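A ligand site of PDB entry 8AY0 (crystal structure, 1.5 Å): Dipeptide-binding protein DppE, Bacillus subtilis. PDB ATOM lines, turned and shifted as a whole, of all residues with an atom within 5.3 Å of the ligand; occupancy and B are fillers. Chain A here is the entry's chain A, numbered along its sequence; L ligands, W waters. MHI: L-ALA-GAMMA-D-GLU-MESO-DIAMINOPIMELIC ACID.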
ATOM      1  N   GLU A  29      13.280  -9.833  10.951  1.00  0.00           N
ATOM      2  CA  GLU A  29      12.971 -11.093  10.289  1.00  0.00           C
ATOM      3  C   GLU A  29      11.508 -11.264   9.943  1.00  0.00           C
ATOM      4  O   GLU A  29      11.200 -11.853   8.914  1.00  0.00           O
ATOM      5  CB  GLU A  29      13.436 -12.287  11.129  1.00  0.00           C
ATOM      6  CG  GLU A  29      14.904 -12.237  11.372  1.00  0.00           C
ATOM      7  CD  GLU A  29      15.439 -13.595  11.770  1.00  0.00           C
ATOM      8  OE1 GLU A  29      15.130 -14.006  12.908  1.00  0.00           O
ATOM      9  OE2 GLU A  29      16.127 -14.229  10.901  1.00  0.00           O
ATOM     10  N   PHE A  41       5.135 -11.075  23.999  1.00  0.00           N
ATOM     11  CA  PHE A  41       5.774 -12.032  24.866  1.00  0.00           C
ATOM     12  C   PHE A  41       6.732 -12.897  24.050  1.00  0.00           C
ATOM     13  O   PHE A  41       6.818 -14.095  24.281  1.00  0.00           O
ATOM     14  CB  PHE A  41       4.754 -12.847  25.663  1.00  0.00           C
ATOM     15  CG  PHE A  41       5.295 -13.552  26.881  1.00  0.00           C
ATOM     16  CD1 PHE A  41       6.274 -12.971  27.651  1.00  0.00           C
ATOM     17  CD2 PHE A  41       4.738 -14.738  27.333  1.00  0.00           C
ATOM     18  CE1 PHE A  41       6.736 -13.565  28.818  1.00  0.00           C
ATOM     19  CE2 PHE A  41       5.254 -15.364  28.462  1.00  0.00           C
ATOM     20  CZ  PHE A  41       6.195 -14.740  29.229  1.00  0.00           C
ATOM     21  N   ASN A  42       7.484 -12.247  23.172  1.00  0.00           N
ATOM     22  CA  ASN A  42       8.390 -12.977  22.285  1.00  0.00           C
ATOM     23  C   ASN A  42       9.379 -11.979  21.706  1.00  0.00           C
ATOM     24  O   ASN A  42       9.196 -10.777  21.771  1.00  0.00           O
ATOM     25  CB  ASN A  42       7.595 -13.807  21.269  1.00  0.00           C
ATOM     26  CG  ASN A  42       6.698 -12.998  20.352  1.00  0.00           C
ATOM     27  OD1 ASN A  42       6.952 -11.821  20.108  1.00  0.00           O
ATOM     28  ND2 ASN A  42       5.638 -13.601  19.858  1.00  0.00           N
ATOM     29  N   ASN A  43      10.459 -12.492  21.149  1.00  0.00           N
ATOM     30  CA  ASN A  43      11.537 -11.701  20.599  1.00  0.00           C
ATOM     31  C   ASN A  43      11.044 -10.863  19.422  1.00  0.00           C
ATOM     32  O   ASN A  43      11.399  -9.695  19.293  1.00  0.00           O
ATOM     33  CB  ASN A  43      12.690 -12.634  20.200  1.00  0.00           C
ATOM     34  CG  ASN A  43      14.052 -12.004  20.235  1.00  0.00           C
ATOM     35  OD1 ASN A  43      14.395 -11.367  21.216  1.00  0.00           O
ATOM     36  ND2 ASN A  43      14.859 -12.213  19.184  1.00  0.00           N
ATOM     37  N   VAL A  44      10.177 -11.420  18.593  1.00  0.00           N
ATOM     38  CA  VAL A  44       9.850 -10.739  17.345  1.00  0.00           C
ATOM     39  C   VAL A  44       9.070  -9.463  17.661  1.00  0.00           C
ATOM     40  O   VAL A  44       9.184  -8.481  16.927  1.00  0.00           O
ATOM     41  CB  VAL A  44       9.158 -11.667  16.339  1.00  0.00           C
ATOM     42  CG1 VAL A  44       7.776 -12.162  16.772  1.00  0.00           C
ATOM     43  CG2 VAL A  44       9.100 -11.019  14.971  1.00  0.00           C
ATOM     44  N   TRP A  46       9.065  -8.014  20.966  1.00  0.00           N
ATOM     45  CA  TRP A  46       9.654  -7.217  22.033  1.00  0.00           C
ATOM     46  C   TRP A  46      11.005  -6.587  21.702  1.00  0.00           C
ATOM     47  O   TRP A  46      11.401  -5.626  22.367  1.00  0.00           O
ATOM     48  CB  TRP A  46       9.662  -8.008  23.342  1.00  0.00           C
ATOM     49  CG  TRP A  46       8.308  -8.099  23.964  1.00  0.00           C
ATOM     50  CD1 TRP A  46       7.155  -7.486  23.551  1.00  0.00           C
ATOM     51  CD2 TRP A  46       7.975  -8.746  25.202  1.00  0.00           C
ATOM     52  NE1 TRP A  46       6.146  -7.725  24.445  1.00  0.00           N
ATOM     53  CE2 TRP A  46       6.624  -8.499  25.465  1.00  0.00           C
ATOM     54  CE3 TRP A  46       8.716  -9.517  26.111  1.00  0.00           C
ATOM     55  CZ2 TRP A  46       5.990  -8.984  26.617  1.00  0.00           C
ATOM     56  CZ3 TRP A  46       8.098 -10.016  27.217  1.00  0.00           C
ATOM     57  CH2 TRP A  46       6.759  -9.721  27.481  1.00  0.00           C
ATOM     58  N   ARG A 237      17.943 -16.169   6.540  1.00  0.00           N
ATOM     59  CA  ARG A 237      19.247 -15.742   7.049  1.00  0.00           C
ATOM     60  C   ARG A 237      20.290 -15.714   5.925  1.00  0.00           C
ATOM     61  O   ARG A 237      21.299 -15.000   6.025  1.00  0.00           O
ATOM     62  CB  ARG A 237      19.604 -16.576   8.290  1.00  0.00           C
ATOM     63  CG  ARG A 237      18.582 -16.415   9.417  1.00  0.00           C
ATOM     64  CD  ARG A 237      19.085 -16.510  10.847  1.00  0.00           C
ATOM     65  NE  ARG A 237      17.988 -16.235  11.792  1.00  0.00           N
ATOM     66  CZ  ARG A 237      18.029 -16.386  13.119  1.00  0.00           C
ATOM     67  NH1 ARG A 237      19.143 -16.710  13.735  1.00  0.00           N
ATOM     68  NH2 ARG A 237      16.920 -16.204  13.825  1.00  0.00           N
ATOM     69  N   TYR A 253      23.037 -12.042  10.810  1.00  0.00           N
ATOM     70  CA  TYR A 253      23.330 -13.375  11.318  1.00  0.00           C
ATOM     71  C   TYR A 253      24.568 -13.920  10.593  1.00  0.00           C
ATOM     72  O   TYR A 253      24.951 -13.407   9.536  1.00  0.00           O
ATOM     73  CB  TYR A 253      22.072 -14.240  11.182  1.00  0.00           C
ATOM     74  CG  TYR A 253      20.899 -13.733  11.984  1.00  0.00           C
ATOM     75  CD1 TYR A 253      20.750 -14.073  13.329  1.00  0.00           C
ATOM     76  CD2 TYR A 253      19.946 -12.865  11.436  1.00  0.00           C
ATOM     77  CE1 TYR A 253      19.676 -13.622  14.083  1.00  0.00           C
ATOM     78  CE2 TYR A 253      18.879 -12.377  12.192  1.00  0.00           C
ATOM     79  CZ  TYR A 253      18.737 -12.780  13.515  1.00  0.00           C
ATOM     80  OH  TYR A 253      17.689 -12.372  14.335  1.00  0.00           O
ATOM     81  N   GLN A 273      23.249 -15.529  25.308  1.00  0.00           N
ATOM     82  CA  GLN A 273      21.809 -15.408  25.449  1.00  0.00           C
ATOM     83  C   GLN A 273      21.291 -16.655  26.154  1.00  0.00           C
ATOM     84  O   GLN A 273      21.455 -17.772  25.637  1.00  0.00           O
ATOM     85  CB  GLN A 273      21.120 -15.246  24.101  1.00  0.00           C
ATOM     86  CG  GLN A 273      19.617 -15.097  24.224  1.00  0.00           C
ATOM     87  CD  GLN A 273      19.026 -14.677  22.904  1.00  0.00           C
ATOM     88  OE1 GLN A 273      19.089 -15.414  21.914  1.00  0.00           O
ATOM     89  NE2 GLN A 273      18.418 -13.496  22.889  1.00  0.00           N
ATOM     90  N   ARG A 280       8.132 -29.732  22.183  1.00  0.00           N
ATOM     91  CA  ARG A 280       7.089 -30.118  23.101  1.00  0.00           C
ATOM     92  C   ARG A 280       6.296 -31.289  22.535  1.00  0.00           C
ATOM     93  O   ARG A 280       5.973 -31.290  21.328  1.00  0.00           O
ATOM     94  CB  ARG A 280       6.108 -28.966  23.302  1.00  0.00           C
ATOM     95  CG  ARG A 280       6.558 -27.896  24.292  1.00  0.00           C
ATOM     96  CD  ARG A 280       5.511 -26.804  24.346  1.00  0.00           C
ATOM     97  NE  ARG A 280       5.937 -25.736  25.241  1.00  0.00           N
ATOM     98  CZ  ARG A 280       6.316 -24.523  24.907  1.00  0.00           C
ATOM     99  NH1 ARG A 280       6.645 -24.218  23.666  1.00  0.00           N
ATOM    100  NH2 ARG A 280       6.410 -23.603  25.892  1.00  0.00           N
ATOM    101  N   LYS A 375       9.986 -21.057   8.608  1.00  0.00           N
ATOM    102  CA  LYS A 375      11.263 -20.357   8.604  1.00  0.00           C
ATOM    103  C   LYS A 375      12.351 -21.358   8.227  1.00  0.00           C
ATOM    104  O   LYS A 375      12.310 -22.503   8.707  1.00  0.00           O
ATOM    105  CB  LYS A 375      11.588 -19.723   9.943  1.00  0.00           C
ATOM    106  CG  LYS A 375      12.610 -18.609   9.933  1.00  0.00           C
ATOM    107  CD  LYS A 375      12.639 -17.984  11.285  1.00  0.00           C
ATOM    108  CE  LYS A 375      13.386 -16.684  11.443  1.00  0.00           C
ATOM    109  NZ  LYS A 375      13.414 -16.354  12.900  1.00  0.00           N
ATOM    110  N   HIS A 378      14.023 -23.451  11.063  1.00  0.00           N
ATOM    111  CA  HIS A 378      13.155 -24.398  11.754  1.00  0.00           C
ATOM    112  C   HIS A 378      12.894 -25.617  10.886  1.00  0.00           C
ATOM    113  O   HIS A 378      12.739 -26.734  11.385  1.00  0.00           O
ATOM    114  CB  HIS A 378      11.849 -23.745  12.224  1.00  0.00           C
ATOM    115  CG  HIS A 378      12.177 -22.609  13.141  1.00  0.00           C
ATOM    116  ND1 HIS A 378      13.092 -22.786  14.174  1.00  0.00           N
ATOM    117  CD2 HIS A 378      11.773 -21.319  13.205  1.00  0.00           C
ATOM    118  CE1 HIS A 378      13.199 -21.631  14.846  1.00  0.00           C
ATOM    119  NE2 HIS A 378      12.400 -20.725  14.272  1.00  0.00           N
ATOM    120  N   TRP A 404       4.660 -18.079  12.505  1.00  0.00           N
ATOM    121  CA  TRP A 404       4.846 -17.998  13.950  1.00  0.00           C
ATOM    122  C   TRP A 404       3.611 -17.480  14.662  1.00  0.00           C
ATOM    123  O   TRP A 404       3.228 -18.005  15.690  1.00  0.00           O
ATOM    124  CB  TRP A 404       6.044 -17.094  14.196  1.00  0.00           C
ATOM    125  CG  TRP A 404       6.484 -16.859  15.600  1.00  0.00           C
ATOM    126  CD1 TRP A 404       6.738 -15.615  16.129  1.00  0.00           C
ATOM    127  CD2 TRP A 404       6.910 -17.813  16.583  1.00  0.00           C
ATOM    128  NE1 TRP A 404       7.245 -15.745  17.395  1.00  0.00           N
ATOM    129  CE2 TRP A 404       7.344 -17.072  17.715  1.00  0.00           C
ATOM    130  CE3 TRP A 404       6.943 -19.200  16.647  1.00  0.00           C
ATOM    131  CZ2 TRP A 404       7.841 -17.693  18.870  1.00  0.00           C
ATOM    132  CZ3 TRP A 404       7.381 -19.814  17.812  1.00  0.00           C
ATOM    133  CH2 TRP A 404       7.854 -19.062  18.888  1.00  0.00           C
ATOM    134  N   LEU A 408       1.988 -19.955  17.234  1.00  0.00           N
ATOM    135  CA  LEU A 408       1.951 -19.700  18.671  1.00  0.00           C
ATOM    136  C   LEU A 408       0.541 -19.861  19.220  1.00  0.00           C
ATOM    137  O   LEU A 408       0.358 -20.496  20.240  1.00  0.00           O
ATOM    138  CB  LEU A 408       2.470 -18.300  18.997  1.00  0.00           C
ATOM    139  CG  LEU A 408       3.980 -18.130  19.117  1.00  0.00           C
ATOM    140  CD1 LEU A 408       4.310 -16.680  19.353  1.00  0.00           C
ATOM    141  CD2 LEU A 408       4.548 -19.027  20.206  1.00  0.00           C
ATOM    142  N   GLN A 411      -0.271 -23.541  19.263  1.00  0.00           N
ATOM    143  CA  GLN A 411       0.507 -24.242  20.283  1.00  0.00           C
ATOM    144  C   GLN A 411      -0.104 -24.065  21.674  1.00  0.00           C
ATOM    145  O   GLN A 411      -0.345 -25.027  22.393  1.00  0.00           O
ATOM    146  CB  GLN A 411       1.957 -23.782  20.226  1.00  0.00           C
ATOM    147  CG  GLN A 411       2.861 -24.602  21.138  1.00  0.00           C
ATOM    148  CD  GLN A 411       4.285 -24.159  20.978  1.00  0.00           C
ATOM    149  OE1 GLN A 411       4.656 -23.038  21.343  1.00  0.00           O
ATOM    150  NE2 GLN A 411       5.115 -25.082  20.468  1.00  0.00           N
ATOM    151  N   LYS A 412      -0.393 -22.805  22.038  1.00  0.00           N
ATOM    152  CA  LYS A 412      -1.045 -22.483  23.293  1.00  0.00           C
ATOM    153  C   LYS A 412      -2.381 -23.201  23.459  1.00  0.00           C
ATOM    154  O   LYS A 412      -2.727 -23.638  24.560  1.00  0.00           O
ATOM    155  CB  LYS A 412      -1.231 -20.969  23.347  1.00  0.00           C
ATOM    156  CG  LYS A 412       0.035 -20.130  23.494  1.00  0.00           C
ATOM    157  CD  LYS A 412      -0.284 -18.663  23.541  1.00  0.00           C
ATOM    158  CE  LYS A 412       0.916 -17.760  23.568  1.00  0.00           C
ATOM    159  NZ  LYS A 412       0.489 -16.363  23.314  1.00  0.00           N
ATOM    160  N   GLN A 420       7.858 -27.514  17.485  1.00  0.00           N
ATOM    161  CA  GLN A 420       8.980 -26.607  17.661  1.00  0.00           C
ATOM    162  C   GLN A 420       8.661 -25.634  18.788  1.00  0.00           C
ATOM    163  O   GLN A 420       7.543 -25.121  18.837  1.00  0.00           O
ATOM    164  CB  GLN A 420       9.279 -25.854  16.379  1.00  0.00           C
ATOM    165  CG  GLN A 420      10.437 -24.887  16.482  1.00  0.00           C
ATOM    166  CD  GLN A 420      10.033 -23.498  16.030  1.00  0.00           C
ATOM    167  OE1 GLN A 420       9.231 -23.354  15.101  1.00  0.00           O
ATOM    168  NE2 GLN A 420      10.511 -22.486  16.728  1.00  0.00           N
ATOM    169  N   SER A 422      10.453 -22.627  21.826  1.00  0.00           N
ATOM    170  CA  SER A 422      11.538 -21.738  22.227  1.00  0.00           C
ATOM    171  C   SER A 422      11.230 -21.201  23.627  1.00  0.00           C
ATOM    172  O   SER A 422      10.098 -20.812  23.875  1.00  0.00           O
ATOM    173  CB  SER A 422      11.715 -20.599  21.255  1.00  0.00           C
ATOM    174  OG  SER A 422      12.738 -19.745  21.701  1.00  0.00           O
ATOM    175  N   PHE A 423      12.269 -21.078  24.474  1.00  0.00           N
ATOM    176  CA  PHE A 423      12.126 -20.438  25.776  1.00  0.00           C
ATOM    177  C   PHE A 423      13.242 -19.419  25.981  1.00  0.00           C
ATOM    178  O   PHE A 423      14.427 -19.760  25.912  1.00  0.00           O
ATOM    179  CB  PHE A 423      12.098 -21.441  26.931  1.00  0.00           C
ATOM    180  CG  PHE A 423      11.888 -20.800  28.287  1.00  0.00           C
ATOM    181  CD1 PHE A 423      10.600 -20.527  28.728  1.00  0.00           C
ATOM    182  CD2 PHE A 423      12.961 -20.376  29.072  1.00  0.00           C
ATOM    183  CE1 PHE A 423      10.400 -19.901  29.961  1.00  0.00           C
ATOM    184  CE2 PHE A 423      12.746 -19.760  30.292  1.00  0.00           C
ATOM    185  CZ  PHE A 423      11.466 -19.496  30.706  1.00  0.00           C
ATOM    186  N   LEU A 424      12.856 -18.166  26.293  1.00  0.00           N
ATOM    187  CA  LEU A 424      13.770 -17.159  26.808  1.00  0.00           C
ATOM    188  C   LEU A 424      13.310 -16.829  28.234  1.00  0.00           C
ATOM    189  O   LEU A 424      12.147 -16.515  28.462  1.00  0.00           O
ATOM    190  CB  LEU A 424      13.710 -15.894  25.938  1.00  0.00           C
ATOM    191  CG  LEU A 424      14.132 -16.028  24.470  1.00  0.00           C
ATOM    192  CD1 LEU A 424      13.832 -14.731  23.697  1.00  0.00           C
ATOM    193  CD2 LEU A 424      15.610 -16.376  24.380  1.00  0.00           C
ATOM    194  N   PRO A 425      14.201 -16.824  29.234  1.00  0.00           N
ATOM    195  CA  PRO A 425      13.808 -16.459  30.584  1.00  0.00           C
ATOM    196  C   PRO A 425      13.444 -14.973  30.653  1.00  0.00           C
ATOM    197  O   PRO A 425      13.954 -14.125  29.918  1.00  0.00           O
ATOM    198  CB  PRO A 425      15.044 -16.751  31.451  1.00  0.00           C
ATOM    199  CG  PRO A 425      16.198 -16.617  30.441  1.00  0.00           C
ATOM    200  CD  PRO A 425      15.634 -17.136  29.129  1.00  0.00           C
ATOM    201  N   ASP A 426      12.561 -14.673  31.629  1.00  0.00           N
ATOM    202  CA  ASP A 426      12.049 -13.318  31.823  1.00  0.00           C
ATOM    203  C   ASP A 426      12.836 -12.586  32.910  1.00  0.00           C
ATOM    204  O   ASP A 426      12.707 -11.355  33.029  1.00  0.00           O
ATOM    205  CB  ASP A 426      10.582 -13.388  32.202  1.00  0.00           C
ATOM    206  CG  ASP A 426       9.758 -14.141  31.175  1.00  0.00           C
ATOM    207  OD1 ASP A 426       9.921 -13.868  29.955  1.00  0.00           O
ATOM    208  OD2 ASP A 426       8.952 -14.991  31.592  1.00  0.00           O
ATOM    209  N   MET A 443       3.169 -21.203  29.764  1.00  0.00           N
ATOM    210  CA  MET A 443       4.403 -21.597  29.078  1.00  0.00           C
ATOM    211  C   MET A 443       4.609 -23.099  29.115  1.00  0.00           C
ATOM    212  O   MET A 443       5.659 -23.589  28.663  1.00  0.00           O
ATOM    213  CB  MET A 443       5.621 -20.903  29.695  1.00  0.00           C
ATOM    214  CG  MET A 443       5.412 -19.436  29.845  1.00  0.00           C
ATOM    215  SD  MET A 443       4.972 -18.622  28.352  1.00  0.00           S
ATOM    216  CE  MET A 443       6.434 -18.911  27.368  1.00  0.00           C
ATOM    217  N   ARG A 445       2.041 -25.802  27.813  1.00  0.00           N
ATOM    218  CA  ARG A 445       1.575 -26.105  26.455  1.00  0.00           C
ATOM    219  C   ARG A 445       1.770 -27.578  26.060  1.00  0.00           C
ATOM    220  O   ARG A 445       1.771 -27.868  24.865  1.00  0.00           O
ATOM    221  CB  ARG A 445       2.225 -25.217  25.390  1.00  0.00           C
ATOM    222  CG  ARG A 445       2.307 -23.736  25.753  1.00  0.00           C
ATOM    223  CD  ARG A 445       2.800 -22.871  24.643  1.00  0.00           C
ATOM    224  NE  ARG A 445       3.072 -21.515  25.131  1.00  0.00           N
ATOM    225  CZ  ARG A 445       3.824 -20.637  24.500  1.00  0.00           C
ATOM    226  NH1 ARG A 445       4.317 -20.888  23.291  1.00  0.00           N
ATOM    227  NH2 ARG A 445       4.062 -19.452  25.063  1.00  0.00           N
ATOM    228  N   TYR A 490      19.032 -27.244  21.854  1.00  0.00           N
ATOM    229  CA  TYR A 490      20.255 -26.493  22.014  1.00  0.00           C
ATOM    230  C   TYR A 490      20.023 -25.207  22.797  1.00  0.00           C
ATOM    231  O   TYR A 490      18.933 -24.673  22.770  1.00  0.00           O
ATOM    232  CB  TYR A 490      20.946 -26.241  20.669  1.00  0.00           C
ATOM    233  CG  TYR A 490      20.300 -25.233  19.739  1.00  0.00           C
ATOM    234  CD1 TYR A 490      20.556 -23.880  19.936  1.00  0.00           C
ATOM    235  CD2 TYR A 490      19.490 -25.598  18.681  1.00  0.00           C
ATOM    236  CE1 TYR A 490      19.971 -22.924  19.132  1.00  0.00           C
ATOM    237  CE2 TYR A 490      18.923 -24.647  17.851  1.00  0.00           C
ATOM    238  CZ  TYR A 490      19.182 -23.303  18.053  1.00  0.00           C
ATOM    239  OH  TYR A 490      18.659 -22.301  17.231  1.00  0.00           O
ATOM    240  N   TYR A 492      20.764 -21.220  23.403  1.00  0.00           N
ATOM    241  CA  TYR A 492      20.961 -20.063  22.564  1.00  0.00           C
ATOM    242  C   TYR A 492      22.314 -19.386  22.824  1.00  0.00           C
ATOM    243  O   TYR A 492      23.005 -19.617  23.820  1.00  0.00           O
ATOM    244  CB  TYR A 492      19.808 -19.068  22.790  1.00  0.00           C
ATOM    245  CG  TYR A 492      18.476 -19.549  22.255  1.00  0.00           C
ATOM    246  CD1 TYR A 492      18.371 -20.076  20.978  1.00  0.00           C
ATOM    247  CD2 TYR A 492      17.317 -19.479  23.002  1.00  0.00           C
ATOM    248  CE1 TYR A 492      17.172 -20.517  20.464  1.00  0.00           C
ATOM    249  CE2 TYR A 492      16.097 -19.930  22.506  1.00  0.00           C
ATOM    250  CZ  TYR A 492      16.022 -20.449  21.225  1.00  0.00           C
ATOM    251  OH  TYR A 492      14.837 -20.910  20.733  1.00  0.00           O
ATOM    252  N   ASN A 493      22.661 -18.531  21.855  1.00  0.00           N
ATOM    253  CA  ASN A 493      23.630 -17.454  21.960  1.00  0.00           C
ATOM    254  C   ASN A 493      23.170 -16.363  20.978  1.00  0.00           C
ATOM    255  O   ASN A 493      22.174 -16.533  20.281  1.00  0.00           O
ATOM    256  CB  ASN A 493      25.046 -17.958  21.678  1.00  0.00           C
ATOM    257  CG  ASN A 493      25.185 -18.550  20.305  1.00  0.00           C
ATOM    258  OD1 ASN A 493      24.305 -18.350  19.486  1.00  0.00           O
ATOM    259  ND2 ASN A 493      26.227 -19.348  20.068  1.00  0.00           N
ATOM    260  N   GLN A 494      23.901 -15.256  20.905  1.00  0.00           N
ATOM    261  CA  GLN A 494      23.591 -14.215  19.934  1.00  0.00           C
ATOM    262  C   GLN A 494      24.887 -13.915  19.182  1.00  0.00           C
ATOM    263  O   GLN A 494      25.707 -13.110  19.587  1.00  0.00           O
ATOM    264  CB  GLN A 494      23.125 -12.911  20.588  1.00  0.00           C
ATOM    265  CG  GLN A 494      22.207 -13.114  21.766  1.00  0.00           C
ATOM    266  CD  GLN A 494      21.719 -11.776  22.303  1.00  0.00           C
ATOM    267  OE1 GLN A 494      21.179 -10.961  21.558  1.00  0.00           O
ATOM    268  NE2 GLN A 494      21.905 -11.596  23.607  1.00  0.00           N
ATOM    269  N   TYR A 512      15.864  -7.693  26.214  1.00  0.00           N
ATOM    270  CA  TYR A 512      15.707  -7.351  24.810  1.00  0.00           C
ATOM    271  C   TYR A 512      16.693  -6.240  24.447  1.00  0.00           C
ATOM    272  O   TYR A 512      17.171  -5.486  25.282  1.00  0.00           O
ATOM    273  CB  TYR A 512      14.229  -7.040  24.494  1.00  0.00           C
ATOM    274  CG  TYR A 512      13.347  -8.219  24.803  1.00  0.00           C
ATOM    275  CD1 TYR A 512      13.249  -9.291  23.920  1.00  0.00           C
ATOM    276  CD2 TYR A 512      12.818  -8.379  26.085  1.00  0.00           C
ATOM    277  CE1 TYR A 512      12.618 -10.461  24.277  1.00  0.00           C
ATOM    278  CE2 TYR A 512      12.151  -9.540  26.438  1.00  0.00           C
ATOM    279  CZ  TYR A 512      12.048 -10.587  25.535  1.00  0.00           C
ATOM    280  OH  TYR A 512      11.371 -11.758  25.844  1.00  0.00           O
HETATM  281  C1  MHI L   1       9.555 -14.332  26.292  1.00  0.00           C
HETATM  282  N1  MHI L   1       9.491 -15.980  28.145  1.00  0.00           N
HETATM  283  O1  MHI L   1       9.979 -17.631  26.089  1.00  0.00           O
HETATM  284  C2  MHI L   1       8.914 -15.604  26.843  1.00  0.00           C
HETATM  285  N2  MHI L   1       8.322 -16.798  24.811  1.00  0.00           N
HETATM  286  O2  MHI L   1       6.863 -19.425  22.930  1.00  0.00           O
HETATM  287  C3  MHI L   1       9.107 -16.785  25.883  1.00  0.00           C
HETATM  288  N3  MHI L   1      12.164 -17.111  20.898  1.00  0.00           N
HETATM  289  O3  MHI L   1       5.928 -17.620  23.919  1.00  0.00           O
HETATM  290  C4  MHI L   1       8.364 -17.860  23.817  1.00  0.00           C
HETATM  291  N4  MHI L   1      19.348 -16.465  19.361  1.00  0.00           N
HETATM  292  O4  MHI L   1      10.718 -15.406  20.989  1.00  0.00           O
HETATM  293  C5  MHI L   1       6.942 -18.354  23.532  1.00  0.00           C
HETATM  294  O5  MHI L   1      12.287 -18.470  18.496  1.00  0.00           O
HETATM  295  C6  MHI L   1       9.019 -17.402  22.505  1.00  0.00           C
HETATM  296  O6  MHI L   1      12.657 -16.509  17.528  1.00  0.00           O
HETATM  297  C7  MHI L   1      10.510 -17.103  22.677  1.00  0.00           C
HETATM  298  O7  MHI L   1      17.318 -16.096  16.487  1.00  0.00           O
HETATM  299  C8  MHI L   1      11.126 -16.477  21.441  1.00  0.00           C
HETATM  300  O8  MHI L   1      18.383 -17.946  17.250  1.00  0.00           O
HETATM  301  C9  MHI L   1      13.038 -16.626  19.859  1.00  0.00           C
HETATM  302  C10 MHI L   1      12.654 -17.265  18.502  1.00  0.00           C
HETATM  303  C11 MHI L   1      14.496 -16.905  20.214  1.00  0.00           C
HETATM  304  C12 MHI L   1      15.500 -16.359  19.221  1.00  0.00           C
HETATM  305  C13 MHI L   1      16.908 -16.660  19.698  1.00  0.00           C
HETATM  306  C15 MHI L   1      17.904 -16.776  17.382  1.00  0.00           C
HETATM  307  C14 MHI L   1      18.023 -16.150  18.775  1.00  0.00           C
HETATM  308  O   HOH W   1      14.490 -20.406  18.169  1.00  0.00           O
HETATM  309  O   HOH W   2       7.589 -21.250  25.080  1.00  0.00           O
HETATM  310  O   HOH W   3       7.387 -21.961  21.859  1.00  0.00           O
HETATM  311  O   HOH W   4      16.062 -19.645  16.506  1.00  0.00           O
HETATM  312  O   HOH W   5      16.525 -13.601  16.701  1.00  0.00           O
HETATM  313  O   HOH W   6       4.613 -15.595  22.687  1.00  0.00           O
HETATM  314  O   HOH W   7      20.555 -14.163  17.980  1.00  0.00           O
HETATM  315  O   HOH W   8      20.992 -19.029  19.200  1.00  0.00           O
HETATM  316  O   HOH W   9      13.402 -18.064  15.373  1.00  0.00           O
HETATM  317  O   HOH W  10      12.690 -14.074  17.001  1.00  0.00           O
HETATM  318  O   HOH W  11       8.260 -17.323  30.315  1.00  0.00           O
HETATM  319  O   HOH W  12       9.850 -14.377  18.482  1.00  0.00           O
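Asn 42 touches the ligand. CZ2 of Trp 404 touches C6 of the ligand, at 3.8 Å. Leu 408 touches the ligand (CD2 to O2, 3.6 Å). CA of Phe 423 touches O1 of the ligand (3.5 Å). Met 443 touches the ligand. Tyr 492 touches the ligand (CD1 to C13, 3.9 Å). OH of Tyr 512 touches C1 of the ligand (3.2 Å). Hydrophobic or aromatic side chains within 4 Å of the ligand: Phe 41, Trp 404, Leu 408, Phe 423, Leu 424, Met 443 and Tyr 492. Of the 29 residues printed, 16 come within 4 Å of the ligand. The nearest printed residue that does not touch the ligand is Tyr 253 (4.2 Å).
The guanidinium group (NE) of Arg 237 is in salt-bridge range of the side-chain carboxylate (OE2) of Glu 29, 2.9 Å away. The side-chain amide oxygen (OE1) of Gln 411 sits at hydrogen-bond distance from the guanidinium group (NH1) of Arg 445. OG of Ser 422 sits at hydrogen-bond distance from OH of Tyr 492, at 2.6 Å. O of Met 443 sits at hydrogen-bond distance from NH2 of Arg 280 (2.9 Å). The guanidinium group (NH2) of Arg 445 sits close to the side-chain sulfur (SD) of Met 443 (3.5 Å).
An oxygen (O3) of the ligand lies within salt-bridge range of the guanidinium group (NH2) of Arg 445 (2.9 Å). An oxygen (O7) of the ligand lies within salt-bridge range of the guanidinium group of Arg 237, 2.7 Å away. An oxygen (O4) of the ligand is in hydrogen-bond range of the backbone NH (N) of Asn 43. An oxygen (O1) of the ligand is in hydrogen-bond range of the backbone NH (N) of Leu 424 (2.9 Å). N1 of the ligand lies within salt-bridge range of OD1 of Asp 426 (2.8 Å). The backbone carbonyl oxygen of Phe 41 lies within hydrogen-bond range of a nitrogen (N2) of the ligand, at 3.1 Å. N1 of the ligand is in hydrogen-bond range of O of Leu 424. A nitrogen (N4) of the ligand lies within hydrogen-bond range of the backbone carbonyl oxygen of Asn 493. The side-chain amide oxygen (OE1) of Gln 273 sits at hydrogen-bond distance from a nitrogen (N4) of the ligand, at 2.8 Å. OG of Ser 422 lies within hydrogen-bond range of N3 of the ligand.
Water W5 lies within hydrogen-bond range of an oxygen (O7) of the ligand, the side-chain hydroxyl (OH) of Tyr 253 and the side-chain amide nitrogen (ND2) of Asn 43. Water W9 lies within hydrogen-bond range of an oxygen (O6) of the ligand, the side-chain amino group of Lys 375 and a ring nitrogen (NE2) of His 378. Water W3 lies within hydrogen-bond range of an oxygen (O2) of the ligand (2.8 Å), the side-chain amide oxygen (OE1) of Gln 411 (3.0 Å), the guanidinium group (NH1) of Arg 280 (3.0 Å) and the backbone NH (N) of Ser 422 (3.1 Å). Water W2 lies within hydrogen-bond range of NH2 of Arg 280 (2.8 Å), O of Ser 422 (2.8 Å) and O2 of the ligand (2.9 Å). Water W1 lies within hydrogen-bond range of OH of Tyr 492 (2.6 Å) and O5 of the ligand (3.0 Å). Water W8 lies within hydrogen-bond range of O of Asn 493 (3.0 Å) and N4 of the ligand (3.1 Å).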
